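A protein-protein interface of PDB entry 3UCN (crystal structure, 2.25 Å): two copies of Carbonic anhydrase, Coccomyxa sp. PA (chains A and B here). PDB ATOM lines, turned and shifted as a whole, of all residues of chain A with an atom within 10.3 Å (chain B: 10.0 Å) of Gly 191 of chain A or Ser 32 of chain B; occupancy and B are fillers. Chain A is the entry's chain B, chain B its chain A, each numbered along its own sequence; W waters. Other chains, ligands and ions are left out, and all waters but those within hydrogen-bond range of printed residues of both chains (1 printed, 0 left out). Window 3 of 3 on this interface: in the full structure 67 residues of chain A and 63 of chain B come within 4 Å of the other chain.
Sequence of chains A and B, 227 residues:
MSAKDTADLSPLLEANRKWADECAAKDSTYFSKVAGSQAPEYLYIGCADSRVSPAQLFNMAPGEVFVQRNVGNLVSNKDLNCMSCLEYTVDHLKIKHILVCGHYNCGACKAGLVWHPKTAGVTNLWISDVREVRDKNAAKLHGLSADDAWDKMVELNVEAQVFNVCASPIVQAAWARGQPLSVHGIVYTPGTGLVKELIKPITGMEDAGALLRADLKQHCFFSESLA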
ATOM      1  N   ASP A  49     -27.288 -26.137 -27.973  1.00  0.00           N
ATOM      2  CA  ASP A  49     -25.863 -25.728 -27.812  1.00  0.00           C
ATOM      3  C   ASP A  49     -25.395 -25.798 -26.370  1.00  0.00           C
ATOM      4  O   ASP A  49     -26.079 -25.263 -25.501  1.00  0.00           O
ATOM      5  CB  ASP A  49     -25.709 -24.299 -28.310  1.00  0.00           C
ATOM      6  CG  ASP A  49     -24.241 -23.813 -28.284  1.00  0.00           C
ATOM      7  OD1 ASP A  49     -23.687 -23.518 -27.212  1.00  0.00           O
ATOM      8  OD2 ASP A  49     -23.665 -23.754 -29.350  1.00  0.00           O
ATOM      9  N   ARG A  51     -23.233 -24.334 -24.635  1.00  0.00           N
ATOM     10  CA  ARG A  51     -22.908 -23.093 -23.882  1.00  0.00           C
ATOM     11  C   ARG A  51     -24.060 -22.278 -23.308  1.00  0.00           C
ATOM     12  O   ARG A  51     -23.771 -21.260 -22.670  1.00  0.00           O
ATOM     13  CB  ARG A  51     -22.057 -22.147 -24.733  1.00  0.00           C
ATOM     14  CG  ARG A  51     -20.941 -22.925 -25.416  1.00  0.00           C
ATOM     15  CD  ARG A  51     -20.333 -22.149 -26.520  1.00  0.00           C
ATOM     16  NE  ARG A  51     -21.103 -22.274 -27.748  1.00  0.00           N
ATOM     17  CZ  ARG A  51     -20.830 -21.649 -28.879  1.00  0.00           C
ATOM     18  NH1 ARG A  51     -19.753 -20.851 -28.981  1.00  0.00           N
ATOM     19  NH2 ARG A  51     -21.622 -21.815 -29.926  1.00  0.00           N
ATOM     20  N   VAL A  52     -25.328 -22.704 -23.503  1.00  0.00           N
ATOM     21  CA  VAL A  52     -26.501 -21.881 -23.197  1.00  0.00           C
ATOM     22  C   VAL A  52     -27.514 -22.592 -22.281  1.00  0.00           C
ATOM     23  O   VAL A  52     -28.576 -23.143 -22.727  1.00  0.00           O
ATOM     24  CB  VAL A  52     -27.229 -21.419 -24.485  1.00  0.00           C
ATOM     25  CG1 VAL A  52     -28.029 -20.213 -24.210  1.00  0.00           C
ATOM     26  CG2 VAL A  52     -26.252 -21.169 -25.615  1.00  0.00           C
ATOM     27  N   HIS A 103     -28.956 -17.594 -29.998  1.00  0.00           N
ATOM     28  CA  HIS A 103     -27.650 -17.223 -29.464  1.00  0.00           C
ATOM     29  C   HIS A 103     -26.708 -17.049 -30.620  1.00  0.00           C
ATOM     30  O   HIS A 103     -26.776 -17.791 -31.611  1.00  0.00           O
ATOM     31  CB  HIS A 103     -27.078 -18.252 -28.473  1.00  0.00           C
ATOM     32  CG  HIS A 103     -26.772 -19.542 -29.128  1.00  0.00           C
ATOM     33  ND1 HIS A 103     -25.503 -19.886 -29.523  1.00  0.00           N
ATOM     34  CD2 HIS A 103     -27.593 -20.550 -29.550  1.00  0.00           C
ATOM     35  CE1 HIS A 103     -25.548 -21.061 -30.156  1.00  0.00           C
ATOM     36  NE2 HIS A 103     -26.809 -21.479 -30.197  1.00  0.00           N
ATOM     37  N   TYR A 104     -25.821 -16.046 -30.486  1.00  0.00           N
ATOM     38  CA  TYR A 104     -24.803 -15.823 -31.506  1.00  0.00           C
ATOM     39  C   TYR A 104     -23.902 -17.030 -31.511  1.00  0.00           C
ATOM     40  O   TYR A 104     -23.842 -17.773 -30.502  1.00  0.00           O
ATOM     41  CB  TYR A 104     -24.011 -14.506 -31.276  1.00  0.00           C
ATOM     42  CG  TYR A 104     -24.898 -13.338 -31.367  1.00  0.00           C
ATOM     43  CD1 TYR A 104     -25.186 -12.627 -30.244  1.00  0.00           C
ATOM     44  CD2 TYR A 104     -25.518 -12.983 -32.606  1.00  0.00           C
ATOM     45  CE1 TYR A 104     -26.025 -11.533 -30.310  1.00  0.00           C
ATOM     46  CE2 TYR A 104     -26.322 -11.899 -32.711  1.00  0.00           C
ATOM     47  CZ  TYR A 104     -26.585 -11.174 -31.548  1.00  0.00           C
ATOM     48  OH  TYR A 104     -27.397 -10.062 -31.556  1.00  0.00           O
ATOM     49  N   ASN A 105     -23.263 -17.227 -32.662  1.00  0.00           N
ATOM     50  CA  ASN A 105     -22.353 -18.385 -32.869  1.00  0.00           C
ATOM     51  C   ASN A 105     -23.129 -19.712 -32.973  1.00  0.00           C
ATOM     52  O   ASN A 105     -22.587 -20.791 -32.704  1.00  0.00           O
ATOM     53  CB  ASN A 105     -21.156 -18.429 -31.869  1.00  0.00           C
ATOM     54  CG  ASN A 105     -20.007 -19.358 -32.364  1.00  0.00           C
ATOM     55  OD1 ASN A 105     -19.667 -20.365 -31.732  1.00  0.00           O
ATOM     56  ND2 ASN A 105     -19.491 -19.076 -33.531  1.00  0.00           N
ATOM     57  N   CYS A 106     -24.407 -19.604 -33.406  1.00  0.00           N
ATOM     58  CA  CYS A 106     -25.315 -20.773 -33.443  1.00  0.00           C
ATOM     59  C   CYS A 106     -25.042 -21.556 -34.666  1.00  0.00           C
ATOM     60  O   CYS A 106     -25.306 -21.046 -35.803  1.00  0.00           O
ATOM     61  CB  CYS A 106     -26.832 -20.344 -33.390  1.00  0.00           C
ATOM     62  SG  CYS A 106     -27.985 -21.820 -33.495  1.00  0.00           S
ATOM     63  N   VAL A 187     -31.550 -12.901 -27.002  1.00  0.00           N
ATOM     64  CA  VAL A 187     -30.431 -13.557 -27.656  1.00  0.00           C
ATOM     65  C   VAL A 187     -29.295 -13.590 -26.625  1.00  0.00           C
ATOM     66  O   VAL A 187     -29.167 -12.714 -25.748  1.00  0.00           O
ATOM     67  CB  VAL A 187     -30.108 -12.866 -28.972  1.00  0.00           C
ATOM     68  CG1 VAL A 187     -29.765 -11.461 -28.702  1.00  0.00           C
ATOM     69  CG2 VAL A 187     -28.982 -13.529 -29.661  1.00  0.00           C
ATOM     70  N   TYR A 188     -28.558 -14.675 -26.595  1.00  0.00           N
ATOM     71  CA  TYR A 188     -27.453 -14.823 -25.631  1.00  0.00           C
ATOM     72  C   TYR A 188     -26.135 -14.716 -26.421  1.00  0.00           C
ATOM     73  O   TYR A 188     -26.084 -15.177 -27.557  1.00  0.00           O
ATOM     74  CB  TYR A 188     -27.582 -16.192 -25.013  1.00  0.00           C
ATOM     75  CG  TYR A 188     -26.510 -16.599 -24.022  1.00  0.00           C
ATOM     76  CD1 TYR A 188     -26.500 -16.120 -22.710  1.00  0.00           C
ATOM     77  CD2 TYR A 188     -25.520 -17.507 -24.406  1.00  0.00           C
ATOM     78  CE1 TYR A 188     -25.462 -16.548 -21.772  1.00  0.00           C
ATOM     79  CE2 TYR A 188     -24.548 -17.947 -23.524  1.00  0.00           C
ATOM     80  CZ  TYR A 188     -24.496 -17.460 -22.208  1.00  0.00           C
ATOM     81  OH  TYR A 188     -23.494 -17.990 -21.361  1.00  0.00           O
ATOM     82  N   THR A 189     -25.107 -14.092 -25.840  1.00  0.00           N
ATOM     83  CA  THR A 189     -23.752 -14.096 -26.468  1.00  0.00           C
ATOM     84  C   THR A 189     -22.873 -15.038 -25.657  1.00  0.00           C
ATOM     85  O   THR A 189     -22.581 -14.777 -24.489  1.00  0.00           O
ATOM     86  CB  THR A 189     -23.122 -12.643 -26.528  1.00  0.00           C
ATOM     87  OG1 THR A 189     -24.051 -11.784 -27.192  1.00  0.00           O
ATOM     88  CG2 THR A 189     -21.778 -12.604 -27.336  1.00  0.00           C
ATOM     89  N   PRO A 190     -22.476 -16.154 -26.248  1.00  0.00           N
ATOM     90  CA  PRO A 190     -21.728 -17.163 -25.451  1.00  0.00           C
ATOM     91  C   PRO A 190     -20.356 -16.639 -24.897  1.00  0.00           C
ATOM     92  O   PRO A 190     -19.910 -17.065 -23.800  1.00  0.00           O
ATOM     93  CB  PRO A 190     -21.465 -18.292 -26.478  1.00  0.00           C
ATOM     94  CG  PRO A 190     -22.540 -18.125 -27.509  1.00  0.00           C
ATOM     95  CD  PRO A 190     -22.776 -16.624 -27.608  1.00  0.00           C
ATOM     96  N   GLY A 191     -19.725 -15.746 -25.676  1.00  0.00           N
ATOM     97  CA  GLY A 191     -18.462 -15.123 -25.351  1.00  0.00           C
ATOM     98  C   GLY A 191     -18.477 -14.219 -24.132  1.00  0.00           C
ATOM     99  O   GLY A 191     -17.409 -13.892 -23.573  1.00  0.00           O
ATOM    100  N   THR A 192     -19.646 -13.769 -23.702  1.00  0.00           N
ATOM    101  CA  THR A 192     -19.681 -12.821 -22.583  1.00  0.00           C
ATOM    102  C   THR A 192     -20.627 -13.267 -21.511  1.00  0.00           C
ATOM    103  O   THR A 192     -20.706 -12.629 -20.442  1.00  0.00           O
ATOM    104  CB  THR A 192     -20.177 -11.429 -23.043  1.00  0.00           C
ATOM    105  OG1 THR A 192     -21.504 -11.562 -23.539  1.00  0.00           O
ATOM    106  CG2 THR A 192     -19.266 -10.816 -24.165  1.00  0.00           C
ATOM    107  N   GLY A 193     -21.402 -14.332 -21.777  1.00  0.00           N
ATOM    108  CA  GLY A 193     -22.443 -14.758 -20.792  1.00  0.00           C
ATOM    109  C   GLY A 193     -23.660 -13.854 -20.655  1.00  0.00           C
ATOM    110  O   GLY A 193     -24.484 -14.010 -19.697  1.00  0.00           O
ATOM    111  N   LEU A 194     -23.801 -12.906 -21.574  1.00  0.00           N
ATOM    112  CA  LEU A 194     -24.871 -11.905 -21.428  1.00  0.00           C
ATOM    113  C   LEU A 194     -26.042 -12.140 -22.386  1.00  0.00           C
ATOM    114  O   LEU A 194     -25.832 -12.552 -23.529  1.00  0.00           O
ATOM    115  CB  LEU A 194     -24.328 -10.480 -21.695  1.00  0.00           C
ATOM    116  CG  LEU A 194     -23.409  -9.909 -20.627  1.00  0.00           C
ATOM    117  CD1 LEU A 194     -22.853  -8.596 -21.123  1.00  0.00           C
ATOM    118  CD2 LEU A 194     -24.217  -9.713 -19.348  1.00  0.00           C
ATOM    119  N   VAL A 195     -27.239 -11.836 -21.894  1.00  0.00           N
ATOM    120  CA  VAL A 195     -28.492 -11.867 -22.639  1.00  0.00           C
ATOM    121  C   VAL A 195     -28.865 -10.449 -23.011  1.00  0.00           C
ATOM    122  O   VAL A 195     -28.740  -9.580 -22.175  1.00  0.00           O
ATOM    123  CB  VAL A 195     -29.658 -12.386 -21.702  1.00  0.00           C
ATOM    124  CG1 VAL A 195     -31.043 -12.181 -22.334  1.00  0.00           C
ATOM    125  CG2 VAL A 195     -29.454 -13.872 -21.322  1.00  0.00           C
ATOM    126  N   TRP B  19     -24.671 -12.546 -12.614  1.00  0.00           N
ATOM    127  CA  TRP B  19     -24.077 -13.865 -12.736  1.00  0.00           C
ATOM    128  C   TRP B  19     -22.884 -13.852 -13.676  1.00  0.00           C
ATOM    129  O   TRP B  19     -21.832 -14.400 -13.320  1.00  0.00           O
ATOM    130  CB  TRP B  19     -25.111 -14.928 -13.174  1.00  0.00           C
ATOM    131  CG  TRP B  19     -24.502 -16.254 -13.714  1.00  0.00           C
ATOM    132  CD1 TRP B  19     -24.131 -17.310 -12.959  1.00  0.00           C
ATOM    133  CD2 TRP B  19     -24.232 -16.628 -15.080  1.00  0.00           C
ATOM    134  NE1 TRP B  19     -23.619 -18.306 -13.747  1.00  0.00           N
ATOM    135  CE2 TRP B  19     -23.702 -17.936 -15.054  1.00  0.00           C
ATOM    136  CE3 TRP B  19     -24.426 -16.012 -16.310  1.00  0.00           C
ATOM    137  CZ2 TRP B  19     -23.324 -18.633 -16.204  1.00  0.00           C
ATOM    138  CZ3 TRP B  19     -24.043 -16.705 -17.478  1.00  0.00           C
ATOM    139  CH2 TRP B  19     -23.518 -18.004 -17.419  1.00  0.00           C
ATOM    140  N   ALA B  20     -23.038 -13.268 -14.871  1.00  0.00           N
ATOM    141  CA  ALA B  20     -21.927 -13.212 -15.829  1.00  0.00           C
ATOM    142  C   ALA B  20     -20.664 -12.523 -15.231  1.00  0.00           C
ATOM    143  O   ALA B  20     -19.526 -12.956 -15.469  1.00  0.00           O
ATOM    144  CB  ALA B  20     -22.354 -12.514 -17.122  1.00  0.00           C
ATOM    145  N   CYS B  23     -18.864 -14.853 -12.543  1.00  0.00           N
ATOM    146  CA  CYS B  23     -18.064 -15.925 -13.154  1.00  0.00           C
ATOM    147  C   CYS B  23     -16.755 -15.405 -13.804  1.00  0.00           C
ATOM    148  O   CYS B  23     -15.681 -16.062 -13.704  1.00  0.00           O
ATOM    149  CB  CYS B  23     -18.863 -16.738 -14.195  1.00  0.00           C
ATOM    150  SG  CYS B  23     -20.310 -17.611 -13.636  1.00  0.00           S
ATOM    151  N   ALA B  24     -16.839 -14.266 -14.500  1.00  0.00           N
ATOM    152  CA  ALA B  24     -15.674 -13.734 -15.238  1.00  0.00           C
ATOM    153  C   ALA B  24     -14.663 -13.144 -14.261  1.00  0.00           C
ATOM    154  O   ALA B  24     -13.468 -13.202 -14.523  1.00  0.00           O
ATOM    155  CB  ALA B  24     -16.075 -12.700 -16.258  1.00  0.00           C
ATOM    156  N   ASP B  27     -12.800 -16.242 -13.007  1.00  0.00           N
ATOM    157  CA  ASP B  27     -11.988 -16.914 -14.043  1.00  0.00           C
ATOM    158  C   ASP B  27     -12.182 -16.080 -15.308  1.00  0.00           C
ATOM    159  O   ASP B  27     -13.284 -16.033 -15.906  1.00  0.00           O
ATOM    160  CB  ASP B  27     -12.389 -18.399 -14.260  1.00  0.00           C
ATOM    161  CG  ASP B  27     -11.716 -19.055 -15.514  1.00  0.00           C
ATOM    162  OD1 ASP B  27     -11.991 -20.253 -15.809  1.00  0.00           O
ATOM    163  OD2 ASP B  27     -10.923 -18.407 -16.235  1.00  0.00           O
ATOM    164  N   SER B  28     -11.124 -15.416 -15.733  1.00  0.00           N
ATOM    165  CA  SER B  28     -11.306 -14.366 -16.710  1.00  0.00           C
ATOM    166  C   SER B  28     -11.601 -14.921 -18.113  1.00  0.00           C
ATOM    167  O   SER B  28     -11.989 -14.147 -18.990  1.00  0.00           O
ATOM    168  CB  SER B  28     -10.095 -13.427 -16.743  1.00  0.00           C
ATOM    169  OG  SER B  28      -9.135 -13.958 -17.625  1.00  0.00           O
ATOM    170  N   THR B  29     -11.406 -16.229 -18.337  1.00  0.00           N
ATOM    171  CA  THR B  29     -11.663 -16.823 -19.680  1.00  0.00           C
ATOM    172  C   THR B  29     -12.865 -17.778 -19.671  1.00  0.00           C
ATOM    173  O   THR B  29     -13.082 -18.497 -20.624  1.00  0.00           O
ATOM    174  CB  THR B  29     -10.459 -17.643 -20.232  1.00  0.00           C
ATOM    175  OG1 THR B  29     -10.037 -18.558 -19.206  1.00  0.00           O
ATOM    176  CG2 THR B  29      -9.338 -16.734 -20.691  1.00  0.00           C
ATOM    177  N   TYR B  30     -13.574 -17.801 -18.547  1.00  0.00           N
ATOM    178  CA  TYR B  30     -14.789 -18.559 -18.385  1.00  0.00           C
ATOM    179  C   TYR B  30     -15.685 -18.563 -19.628  1.00  0.00           C
ATOM    180  O   TYR B  30     -16.124 -19.625 -20.055  1.00  0.00           O
ATOM    181  CB  TYR B  30     -15.588 -17.991 -17.258  1.00  0.00           C
ATOM    182  CG  TYR B  30     -16.617 -18.941 -16.738  1.00  0.00           C
ATOM    183  CD1 TYR B  30     -16.238 -20.034 -15.910  1.00  0.00           C
ATOM    184  CD2 TYR B  30     -17.976 -18.725 -16.988  1.00  0.00           C
ATOM    185  CE1 TYR B  30     -17.194 -20.873 -15.368  1.00  0.00           C
ATOM    186  CE2 TYR B  30     -18.935 -19.557 -16.446  1.00  0.00           C
ATOM    187  CZ  TYR B  30     -18.552 -20.621 -15.644  1.00  0.00           C
ATOM    188  OH  TYR B  30     -19.508 -21.439 -15.118  1.00  0.00           O
ATOM    189  N   PHE B  31     -15.906 -17.390 -20.211  1.00  0.00           N
ATOM    190  CA  PHE B  31     -16.781 -17.262 -21.354  1.00  0.00           C
ATOM    191  C   PHE B  31     -16.013 -17.176 -22.657  1.00  0.00           C
ATOM    192  O   PHE B  31     -16.352 -17.827 -23.652  1.00  0.00           O
ATOM    193  CB  PHE B  31     -17.666 -16.027 -21.163  1.00  0.00           C
ATOM    194  CG  PHE B  31     -18.622 -16.119 -20.008  1.00  0.00           C
ATOM    195  CD1 PHE B  31     -19.640 -17.116 -19.985  1.00  0.00           C
ATOM    196  CD2 PHE B  31     -18.585 -15.207 -18.990  1.00  0.00           C
ATOM    197  CE1 PHE B  31     -20.563 -17.176 -18.926  1.00  0.00           C
ATOM    198  CE2 PHE B  31     -19.499 -15.282 -17.900  1.00  0.00           C
ATOM    199  CZ  PHE B  31     -20.493 -16.292 -17.891  1.00  0.00           C
ATOM    200  N   SER B  32     -14.957 -16.359 -22.666  1.00  0.00           N
ATOM    201  CA  SER B  32     -14.232 -16.000 -23.903  1.00  0.00           C
ATOM    202  C   SER B  32     -13.679 -17.252 -24.563  1.00  0.00           C
ATOM    203  O   SER B  32     -13.506 -17.303 -25.821  1.00  0.00           O
ATOM    204  CB  SER B  32     -13.048 -15.022 -23.561  1.00  0.00           C
ATOM    205  OG  SER B  32     -12.101 -15.611 -22.592  1.00  0.00           O
ATOM    206  N   LYS B  33     -13.330 -18.248 -23.738  1.00  0.00           N
ATOM    207  CA  LYS B  33     -12.741 -19.505 -24.281  1.00  0.00           C
ATOM    208  C   LYS B  33     -13.675 -20.350 -25.205  1.00  0.00           C
ATOM    209  O   LYS B  33     -13.213 -21.131 -26.032  1.00  0.00           O
ATOM    210  CB  LYS B  33     -12.111 -20.349 -23.158  1.00  0.00           C
ATOM    211  CG  LYS B  33     -13.077 -21.089 -22.306  1.00  0.00           C
ATOM    212  CD  LYS B  33     -12.419 -22.052 -21.305  1.00  0.00           C
ATOM    213  CE  LYS B  33     -13.381 -22.096 -20.099  1.00  0.00           C
ATOM    214  NZ  LYS B  33     -13.075 -23.256 -19.222  1.00  0.00           N
ATOM    215  N   VAL B  34     -14.988 -20.125 -25.070  1.00  0.00           N
ATOM    216  CA  VAL B  34     -16.023 -20.793 -25.850  1.00  0.00           C
ATOM    217  C   VAL B  34     -16.826 -19.711 -26.648  1.00  0.00           C
ATOM    218  O   VAL B  34     -18.017 -19.892 -26.913  1.00  0.00           O
ATOM    219  CB  VAL B  34     -17.025 -21.585 -24.892  1.00  0.00           C
ATOM    220  CG1 VAL B  34     -16.306 -22.724 -24.163  1.00  0.00           C
ATOM    221  CG2 VAL B  34     -17.683 -20.674 -23.903  1.00  0.00           C
ATOM    222  N   ALA B  35     -16.178 -18.585 -26.972  1.00  0.00           N
ATOM    223  CA  ALA B  35     -16.813 -17.514 -27.728  1.00  0.00           C
ATOM    224  C   ALA B  35     -17.184 -17.982 -29.111  1.00  0.00           C
ATOM    225  O   ALA B  35     -18.202 -17.521 -29.673  1.00  0.00           O
ATOM    226  CB  ALA B  35     -15.906 -16.258 -27.843  1.00  0.00           C
ATOM    227  N   GLY B  36     -16.362 -18.857 -29.672  1.00  0.00           N
ATOM    228  CA  GLY B  36     -16.401 -19.038 -31.117  1.00  0.00           C
ATOM    229  C   GLY B  36     -16.464 -20.494 -31.409  1.00  0.00           C
ATOM    230  O   GLY B  36     -16.480 -20.883 -32.545  1.00  0.00           O
ATOM    231  N   SER B  37     -16.593 -21.322 -30.373  1.00  0.00           N
ATOM    232  CA  SER B  37     -16.628 -22.744 -30.623  1.00  0.00           C
ATOM    233  C   SER B  37     -17.098 -23.576 -29.388  1.00  0.00           C
ATOM    234  O   SER B  37     -17.205 -23.041 -28.287  1.00  0.00           O
ATOM    235  CB  SER B  37     -15.223 -23.103 -31.086  1.00  0.00           C
ATOM    236  OG  SER B  37     -14.850 -24.380 -30.665  1.00  0.00           O
ATOM    237  N   GLN B  38     -17.425 -24.859 -29.576  1.00  0.00           N
ATOM    238  CA  GLN B  38     -17.801 -25.718 -28.432  1.00  0.00           C
ATOM    239  C   GLN B  38     -17.286 -27.103 -28.747  1.00  0.00           C
ATOM    240  O   GLN B  38     -17.185 -27.486 -29.925  1.00  0.00           O
ATOM    241  CB  GLN B  38     -19.322 -25.798 -28.240  1.00  0.00           C
ATOM    242  CG  GLN B  38     -20.082 -26.507 -29.384  1.00  0.00           C
ATOM    243  CD  GLN B  38     -21.595 -26.653 -29.121  1.00  0.00           C
ATOM    244  OE1 GLN B  38     -22.066 -26.946 -27.989  1.00  0.00           O
ATOM    245  NE2 GLN B  38     -22.359 -26.464 -30.171  1.00  0.00           N
ATOM    246  N   PRO B  62     -20.359 -23.659 -18.886  1.00  0.00           N
ATOM    247  CA  PRO B  62     -20.766 -23.592 -20.294  1.00  0.00           C
ATOM    248  C   PRO B  62     -19.815 -24.386 -21.175  1.00  0.00           C
ATOM    249  O   PRO B  62     -18.591 -24.335 -20.977  1.00  0.00           O
ATOM    250  CB  PRO B  62     -20.596 -22.119 -20.625  1.00  0.00           C
ATOM    251  CG  PRO B  62     -20.860 -21.414 -19.293  1.00  0.00           C
ATOM    252  CD  PRO B  62     -20.275 -22.327 -18.265  1.00  0.00           C
HETATM  253  O   HOH W   1     -19.774 -15.435 -28.356  1.00  0.00           O
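NH1 of Arg 51 of chain A is in hydrogen-bond range of O of Ser 37 of chain B, 3.4 Å away.
The side-chain amide nitrogen (NE2) of Gln 38 of chain B lies within hydrogen-bond range of the side-chain carboxylate (OD2) of Asp 49 of chain A (3.1 Å).
O of Val 34 of chain B sits at hydrogen-bond distance from NH1 of Arg 51 of chain A, at 2.9 Å.
OD1 of Asn 105 of chain A lies within hydrogen-bond range of N of Ser 37 of chain B, 3.5 Å away.
The backbone carbonyl oxygen of Gly 36 of chain B lies close to the side-chain amide oxygen of Asn 105 of chain A, at 3.3 Å.
The backbone carbonyl oxygen (O) of Tyr 188 of chain A sits at hydrogen-bond distance from the backbone NH (N) of Tyr 104 of chain A (3.1 Å).
The side-chain amide oxygen (OD1) of Asn 105 of chain A is in hydrogen-bond range of the guanidinium group (NH1) of Arg 51 of chain A (2.8 Å).
The indole nitrogen (NE1) of Trp 19 of chain B sits at hydrogen-bond distance from the side-chain sulfur (SG) of Cys 23 of chain B (3.4 Å).
The side-chain carboxylate (OD2) of Asp 49 of chain A is in salt-bridge range of the guanidinium group (NH2) of Arg 51 of chain A, 2.9 Å away.
The side-chain hydroxyl (OG1) of Thr 192 of chain A lies close to the backbone NH (N) of Leu 194 of chain A, at 3.3 Å.
O of Ala 35 of chain B touches NH1 of Arg 51 of chain A, 3.7 Å away.
Asn 105 of chain A touches Ala 35 of chain B (CG to O, 3.7 Å).
Trp 19 of chain B touches Tyr 188 of chain A (CH2 to OH, 3.9 Å).
Phe 31 of chain B touches Tyr 188 of chain A.
Phe 31 of chain B touches Pro 190 of chain A.
CB of Pro 190 of chain A touches O of Val 34 of chain B (3.8 Å).
Gly 191 of chain A touches Phe 31 of chain B (O to CB, 3.2 Å).
O of Gly 191 of chain A touches N of Ser 32 of chain B (3.6 Å).
Phe 31 of chain B touches Thr 192 of chain A.
Gly 193 of chain A touches Phe 31 of chain B (CA to CE1, 3.6 Å).
Printed residues of chain B within 4 Å of Arg 51 of chain A: Val 34 (2.9 Å), Ala 35 (3.7 Å), Gly 36 (3.99 Å), Ser 37 (3.4 Å), Gln 38 (3.98 Å) and Pro 62 (3.9 Å).
Printed residues of chain B within 4 Å of Tyr 188 of chain A: Trp 19 and Phe 31.
Pro 190 of chain A touches two residues of chain B.
Gly 191 of chain A touches just these residues of chain B: Phe 31, Ser 32 and Ala 35.
Thr 29 of chain B touches none of the printed residues of chain A.
Printed residues of chain A within 4 Å of Phe 31 of chain B: Tyr 188 (3.9 Å), Pro 190 (3.6 Å), Gly 191 (3.2 Å), Thr 192 (3.6 Å) and Gly 193 (3.6 Å).
Of chain A, only Gly 191 (3.6 Å) comes within 4 Å of Ser 32 of chain B.
Of chain A, only Arg 51 (3.7 Å), Asn 105 (3.7 Å) and Gly 191 (3.7 Å) come within 4 Å of Ala 35 of chain B.
Of the printed residues of chain A, Pro 62 of chain B touches Arg 51.
The nearest residue of chain B that does not touch Gly 191 of chain A is Val 34 of chain B (4.7 Å).
The nearest residue of chain A that does not touch Ser 32 of chain B is Pro 190 of chain A (5.1 Å).
The nearest printed residue of chain A that does not touch Gly 36 of chain B is Pro 190 of chain A (6.0 Å).
Printed residues of chain A that touch a printed residue of chain B: Asp 49, Arg 51, Asn 105, Tyr 188, Pro 190, Gly 191, Thr 192 and Gly 193.
Along chain A the printed residues that touch a printed residue of chain B span positions 49 to 193.
Printed residues of chain B that touch a printed residue of chain A: Trp 19, Ala 20, Phe 31, Ser 32, Val 34, Ala 35, Gly 36, Ser 37, Gln 38 and Pro 62.
Among the printed residues, no Asp or Glu carboxylate lies within 4 Å of a Lys or Arg side-chain nitrogen of the other chain.
No position is printed for both chains.
Of the 22 pairs that touch across the chains among the printed residues, none has its exchanged pair printed and touching as well.
Water W1 bridges N of Gly 191 of chain A and O of Ala 35 of chain B.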
